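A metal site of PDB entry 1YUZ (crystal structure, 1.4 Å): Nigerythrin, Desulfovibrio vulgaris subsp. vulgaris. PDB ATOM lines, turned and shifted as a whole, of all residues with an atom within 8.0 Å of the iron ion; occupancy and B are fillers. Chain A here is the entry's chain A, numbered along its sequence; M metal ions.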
ATOM      1  N   ILE A  75      -1.456   2.997 -12.844  1.00  0.00           N
ATOM      2  CA  ILE A  75      -1.957   2.313 -11.660  1.00  0.00           C
ATOM      3  C   ILE A  75      -1.645   3.191 -10.451  1.00  0.00           C
ATOM      4  O   ILE A  75      -2.487   3.375  -9.572  1.00  0.00           O
ATOM      5  CB  ILE A  75      -1.284   0.923 -11.493  1.00  0.00           C
ATOM      6  CG1 ILE A  75      -1.849  -0.043 -12.529  1.00  0.00           C
ATOM      7  CG2 ILE A  75      -1.519   0.384 -10.078  1.00  0.00           C
ATOM      8  CD1 ILE A  75      -1.182  -1.406 -12.553  1.00  0.00           C
ATOM      9  N   ARG A 144       3.740   1.651  -1.785  1.00  0.00           N
ATOM     10  CA  ARG A 144       3.540   0.737  -2.901  1.00  0.00           C
ATOM     11  C   ARG A 144       4.154   1.320  -4.175  1.00  0.00           C
ATOM     12  O   ARG A 144       4.842   0.626  -4.919  1.00  0.00           O
ATOM     13  CB  ARG A 144       2.041   0.476  -3.082  1.00  0.00           C
ATOM     14  CG  ARG A 144       1.699  -0.576  -4.114  1.00  0.00           C
ATOM     15  CD  ARG A 144       0.429  -1.317  -3.737  1.00  0.00           C
ATOM     16  NE  ARG A 144       0.645  -2.177  -2.570  1.00  0.00           N
ATOM     17  CZ  ARG A 144      -0.245  -3.027  -2.083  1.00  0.00           C
ATOM     18  NH1 ARG A 144      -1.440  -3.153  -2.667  1.00  0.00           N
ATOM     19  NH2 ARG A 144       0.052  -3.780  -1.030  1.00  0.00           N
ATOM     20  N   ALA A 148       7.704   0.074  -6.506  1.00  0.00           N
ATOM     21  CA  ALA A 148       7.655  -0.244  -7.918  1.00  0.00           C
ATOM     22  C   ALA A 148       8.663   0.571  -8.718  1.00  0.00           C
ATOM     23  O   ALA A 148       9.256   0.070  -9.669  1.00  0.00           O
ATOM     24  CB  ALA A 148       6.259  -0.002  -8.468  1.00  0.00           C
ATOM     25  N   LEU A 173       2.768  -7.152 -15.778  1.00  0.00           N
ATOM     26  CA  LEU A 173       2.438  -6.067 -14.869  1.00  0.00           C
ATOM     27  C   LEU A 173       1.404  -6.517 -13.849  1.00  0.00           C
ATOM     28  O   LEU A 173       0.394  -7.123 -14.203  1.00  0.00           O
ATOM     29  CB  LEU A 173       1.898  -4.873 -15.657  1.00  0.00           C
ATOM     30  CG  LEU A 173       1.397  -3.691 -14.820  1.00  0.00           C
ATOM     31  CD1 LEU A 173       2.560  -3.070 -14.045  1.00  0.00           C
ATOM     32  CD2 LEU A 173       0.766  -2.659 -15.745  1.00  0.00           C
ATOM     33  N   CYS A 174       1.653  -6.205 -12.582  1.00  0.00           N
ATOM     34  CA  CYS A 174       0.746  -6.553 -11.512  1.00  0.00           C
ATOM     35  C   CYS A 174      -0.580  -5.819 -11.687  1.00  0.00           C
ATOM     36  O   CYS A 174      -0.609  -4.711 -12.215  1.00  0.00           O
ATOM     37  CB  CYS A 174       1.375  -6.198 -10.165  1.00  0.00           C
ATOM     38  SG  CYS A 174       0.346  -6.529  -8.731  1.00  0.00           S
ATOM     39  N   PRO A 175      -1.686  -6.423 -11.264  1.00  0.00           N
ATOM     40  CA  PRO A 175      -2.990  -5.772 -11.413  1.00  0.00           C
ATOM     41  C   PRO A 175      -3.238  -4.587 -10.475  1.00  0.00           C
ATOM     42  O   PRO A 175      -3.967  -3.668 -10.828  1.00  0.00           O
ATOM     43  CB  PRO A 175      -3.975  -6.915 -11.144  1.00  0.00           C
ATOM     44  CG  PRO A 175      -3.240  -7.750 -10.154  1.00  0.00           C
ATOM     45  CD  PRO A 175      -1.846  -7.794 -10.747  1.00  0.00           C
ATOM     46  N   ILE A 176      -2.614  -4.590  -9.301  1.00  0.00           N
ATOM     47  CA  ILE A 176      -2.835  -3.521  -8.338  1.00  0.00           C
ATOM     48  C   ILE A 176      -1.643  -2.669  -7.932  1.00  0.00           C
ATOM     49  O   ILE A 176      -1.791  -1.717  -7.154  1.00  0.00           O
ATOM     50  CB  ILE A 176      -3.535  -4.060  -7.070  1.00  0.00           C
ATOM     51  CG1 ILE A 176      -2.624  -5.050  -6.352  1.00  0.00           C
ATOM     52  CG2 ILE A 176      -4.847  -4.730  -7.455  1.00  0.00           C
ATOM     53  CD1 ILE A 176      -3.169  -5.521  -5.018  1.00  0.00           C
ATOM     54  N   CYS A 177      -0.453  -3.001  -8.413  1.00  0.00           N
ATOM     55  CA  CYS A 177       0.716  -2.189  -8.105  1.00  0.00           C
ATOM     56  C   CYS A 177       1.571  -2.100  -9.359  1.00  0.00           C
ATOM     57  O   CYS A 177       1.258  -2.740 -10.375  1.00  0.00           O
ATOM     58  CB  CYS A 177       1.501  -2.743  -6.908  1.00  0.00           C
ATOM     59  SG  CYS A 177       2.717  -4.028  -7.224  1.00  0.00           S
ATOM     60  N   GLY A 178       2.632  -1.316  -9.307  1.00  0.00           N
ATOM     61  CA  GLY A 178       3.465  -1.130 -10.477  1.00  0.00           C
ATOM     62  C   GLY A 178       4.523  -2.166 -10.756  1.00  0.00           C
ATOM     63  O   GLY A 178       5.335  -1.992 -11.669  1.00  0.00           O
ATOM     64  N   TYR A 179       4.528  -3.265 -10.011  1.00  0.00           N
ATOM     65  CA  TYR A 179       5.535  -4.291 -10.232  1.00  0.00           C
ATOM     66  C   TYR A 179       5.506  -4.865 -11.648  1.00  0.00           C
ATOM     67  O   TYR A 179       4.452  -5.204 -12.165  1.00  0.00           O
ATOM     68  CB  TYR A 179       5.380  -5.430  -9.238  1.00  0.00           C
ATOM     69  CG  TYR A 179       6.426  -6.502  -9.424  1.00  0.00           C
ATOM     70  CD1 TYR A 179       7.758  -6.263  -9.115  1.00  0.00           C
ATOM     71  CD2 TYR A 179       6.075  -7.754  -9.939  1.00  0.00           C
ATOM     72  CE1 TYR A 179       8.735  -7.233  -9.330  1.00  0.00           C
ATOM     73  CE2 TYR A 179       7.042  -8.733 -10.143  1.00  0.00           C
ATOM     74  CZ  TYR A 179       8.367  -8.462  -9.842  1.00  0.00           C
ATOM     75  OH  TYR A 179       9.316  -9.439 -10.032  1.00  0.00           O
ATOM     76  N   ILE A 180       6.692  -4.966 -12.258  1.00  0.00           N
ATOM     77  CA  ILE A 180       6.822  -5.533 -13.589  1.00  0.00           C
ATOM     78  C   ILE A 180       7.870  -6.631 -13.553  1.00  0.00           C
ATOM     79  O   ILE A 180       8.963  -6.450 -13.022  1.00  0.00           O
ATOM     80  CB  ILE A 180       7.278  -4.464 -14.622  1.00  0.00           C
ATOM     81  CG1 ILE A 180       6.177  -3.421 -14.802  1.00  0.00           C
ATOM     82  CG2 ILE A 180       7.614  -5.135 -15.967  1.00  0.00           C
ATOM     83  CD1 ILE A 180       6.612  -2.211 -15.598  1.00  0.00           C
ATOM     84  N   LYS A 188       4.498 -14.859  -7.795  1.00  0.00           N
ATOM     85  CA  LYS A 188       3.667 -13.764  -7.319  1.00  0.00           C
ATOM     86  C   LYS A 188       4.429 -12.456  -7.236  1.00  0.00           C
ATOM     87  O   LYS A 188       5.657 -12.421  -7.357  1.00  0.00           O
ATOM     88  CB  LYS A 188       3.099 -14.109  -5.941  1.00  0.00           C
ATOM     89  CG  LYS A 188       4.151 -14.294  -4.857  1.00  0.00           C
ATOM     90  CD  LYS A 188       3.496 -14.574  -3.505  1.00  0.00           C
ATOM     91  CE  LYS A 188       4.538 -14.757  -2.420  1.00  0.00           C
ATOM     92  NZ  LYS A 188       3.912 -15.033  -1.092  1.00  0.00           N
ATOM     93  N   CYS A 189       3.684 -11.380  -7.028  1.00  0.00           N
ATOM     94  CA  CYS A 189       4.260 -10.041  -6.915  1.00  0.00           C
ATOM     95  C   CYS A 189       5.007  -9.888  -5.588  1.00  0.00           C
ATOM     96  O   CYS A 189       4.459 -10.162  -4.526  1.00  0.00           O
ATOM     97  CB  CYS A 189       3.150  -9.005  -7.012  1.00  0.00           C
ATOM     98  SG  CYS A 189       3.731  -7.313  -6.908  1.00  0.00           S
ATOM     99  N   PRO A 190       6.270  -9.453  -5.641  1.00  0.00           N
ATOM    100  CA  PRO A 190       7.046  -9.276  -4.410  1.00  0.00           C
ATOM    101  C   PRO A 190       6.641  -8.039  -3.608  1.00  0.00           C
ATOM    102  O   PRO A 190       7.040  -7.885  -2.457  1.00  0.00           O
ATOM    103  CB  PRO A 190       8.476  -9.182  -4.918  1.00  0.00           C
ATOM    104  CG  PRO A 190       8.308  -8.464  -6.215  1.00  0.00           C
ATOM    105  CD  PRO A 190       7.106  -9.177  -6.821  1.00  0.00           C
ATOM    106  N   ILE A 191       5.829  -7.173  -4.222  1.00  0.00           N
ATOM    107  CA  ILE A 191       5.379  -5.962  -3.545  1.00  0.00           C
ATOM    108  C   ILE A 191       4.026  -6.146  -2.847  1.00  0.00           C
ATOM    109  O   ILE A 191       3.872  -5.732  -1.705  1.00  0.00           O
ATOM    110  CB  ILE A 191       5.273  -4.782  -4.546  1.00  0.00           C
ATOM    111  CG1 ILE A 191       6.678  -4.410  -5.049  1.00  0.00           C
ATOM    112  CG2 ILE A 191       4.605  -3.577  -3.874  1.00  0.00           C
ATOM    113  CD1 ILE A 191       6.684  -3.310  -6.099  1.00  0.00           C
ATOM    114  N   CYS A 192       3.072  -6.769  -3.534  1.00  0.00           N
ATOM    115  CA  CYS A 192       1.744  -6.949  -2.942  1.00  0.00           C
ATOM    116  C   CYS A 192       1.294  -8.415  -2.854  1.00  0.00           C
ATOM    117  O   CYS A 192       0.202  -8.685  -2.362  1.00  0.00           O
ATOM    118  CB  CYS A 192       0.708  -6.152  -3.732  1.00  0.00           C
ATOM    119  SG  CYS A 192       0.390  -6.817  -5.375  1.00  0.00           S
ATOM    120  N   PHE A 193       2.122  -9.327  -3.338  1.00  0.00           N
ATOM    121  CA  PHE A 193       1.824 -10.758  -3.295  1.00  0.00           C
ATOM    122  C   PHE A 193       0.759 -11.287  -4.248  1.00  0.00           C
ATOM    123  O   PHE A 193       0.385 -12.462  -4.171  1.00  0.00           O
ATOM    124  CB  PHE A 193       1.480 -11.177  -1.852  1.00  0.00           C
ATOM    125  CG  PHE A 193       2.687 -11.340  -0.967  1.00  0.00           C
ATOM    126  CD1 PHE A 193       3.918 -10.805  -1.319  1.00  0.00           C
ATOM    127  CD2 PHE A 193       2.578 -12.036   0.244  1.00  0.00           C
ATOM    128  CE1 PHE A 193       5.029 -10.944  -0.478  1.00  0.00           C
ATOM    129  CE2 PHE A 193       3.680 -12.173   1.086  1.00  0.00           C
ATOM    130  CZ  PHE A 193       4.911 -11.628   0.724  1.00  0.00           C
ATOM    131  N   ARG A 194       0.256 -10.447  -5.145  1.00  0.00           N
ATOM    132  CA  ARG A 194      -0.747 -10.905  -6.107  1.00  0.00           C
ATOM    133  C   ARG A 194      -0.148 -12.043  -6.950  1.00  0.00           C
ATOM    134  O   ARG A 194       0.982 -11.950  -7.408  1.00  0.00           O
ATOM    135  CB  ARG A 194      -1.184  -9.762  -7.024  1.00  0.00           C
ATOM    136  CG  ARG A 194      -2.366  -8.964  -6.512  1.00  0.00           C
ATOM    137  CD  ARG A 194      -3.651  -9.774  -6.598  1.00  0.00           C
ATOM    138  NE  ARG A 194      -4.846  -8.999  -6.267  1.00  0.00           N
ATOM    139  CZ  ARG A 194      -5.206  -8.681  -5.031  1.00  0.00           C
ATOM    140  NH1 ARG A 194      -4.484  -9.087  -3.986  1.00  0.00           N
ATOM    141  NH2 ARG A 194      -6.308  -7.964  -4.827  1.00  0.00           N
ATOM    142  N   PRO A 195      -0.912 -13.120  -7.153  1.00  0.00           N
ATOM    143  CA  PRO A 195      -0.439 -14.257  -7.955  1.00  0.00           C
ATOM    144  C   PRO A 195      -0.202 -13.902  -9.421  1.00  0.00           C
ATOM    145  O   PRO A 195      -0.871 -13.037  -9.977  1.00  0.00           O
ATOM    146  CB  PRO A 195      -1.546 -15.302  -7.778  1.00  0.00           C
ATOM    147  CG  PRO A 195      -2.130 -14.956  -6.434  1.00  0.00           C
ATOM    148  CD  PRO A 195      -2.194 -13.449  -6.508  1.00  0.00           C
ATOM    149  N   THR A 198      -2.901 -13.166 -12.137  1.00  0.00           N
ATOM    150  CA  THR A 198      -3.670 -11.930 -12.178  1.00  0.00           C
ATOM    151  C   THR A 198      -2.957 -10.815 -12.939  1.00  0.00           C
ATOM    152  O   THR A 198      -3.508  -9.728 -13.128  1.00  0.00           O
ATOM    153  CB  THR A 198      -3.990 -11.422 -10.755  1.00  0.00           C
ATOM    154  OG1 THR A 198      -2.767 -11.096 -10.073  1.00  0.00           O
ATOM    155  CG2 THR A 198      -4.733 -12.491  -9.969  1.00  0.00           C
ATOM    156  N   PHE A 199      -1.724 -11.081 -13.355  1.00  0.00           N
ATOM    157  CA  PHE A 199      -0.916 -10.102 -14.092  1.00  0.00           C
ATOM    158  C   PHE A 199      -1.375  -9.950 -15.536  1.00  0.00           C
ATOM    159  O   PHE A 199      -2.060 -10.825 -16.086  1.00  0.00           O
ATOM    160  CB  PHE A 199       0.556 -10.520 -14.092  1.00  0.00           C
ATOM    161  CG  PHE A 199       1.291 -10.194 -12.823  1.00  0.00           C
ATOM    162  CD1 PHE A 199       0.810 -10.616 -11.580  1.00  0.00           C
ATOM    163  CD2 PHE A 199       2.488  -9.474 -12.874  1.00  0.00           C
ATOM    164  CE1 PHE A 199       1.519 -10.339 -10.418  1.00  0.00           C
ATOM    165  CE2 PHE A 199       3.197  -9.197 -11.712  1.00  0.00           C
ATOM    166  CZ  PHE A 199       2.715  -9.620 -10.480  1.00  0.00           C
HETATM  167 FE    FE M   1       1.738  -6.064  -6.971  1.00  0.00          FE
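The iron ion is bound by the side-chain sulfur (SG) of Cys 192, 2.2 Å away. The iron ion is bound by SG of Cys 177. SG of Cys 174 binds the iron ion, at 2.3 Å. The iron ion is bound by the side-chain sulfur (SG) of Cys 189 (2.4 Å).
The backbone NH of Arg 194 lies close to the side-chain sulfur of Cys 192. N of Tyr 179 sits close to SG of Cys 177, at 3.4 Å. The backbone NH of Cys 174 is in hydrogen-bond range of the backbone carbonyl oxygen of Tyr 179 (3.0 Å). The backbone NH (N) of Ile 176 sits close to the side-chain sulfur (SG) of Cys 174 (3.6 Å). SG of Cys 189 lies close to N of Ile 191 (3.4 Å). O of Arg 194 sits at hydrogen-bond distance from N of Cys 189 (2.8 Å).
The nearest printed residue that does not touch the iron ion is Tyr 179 (4.3 Å).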
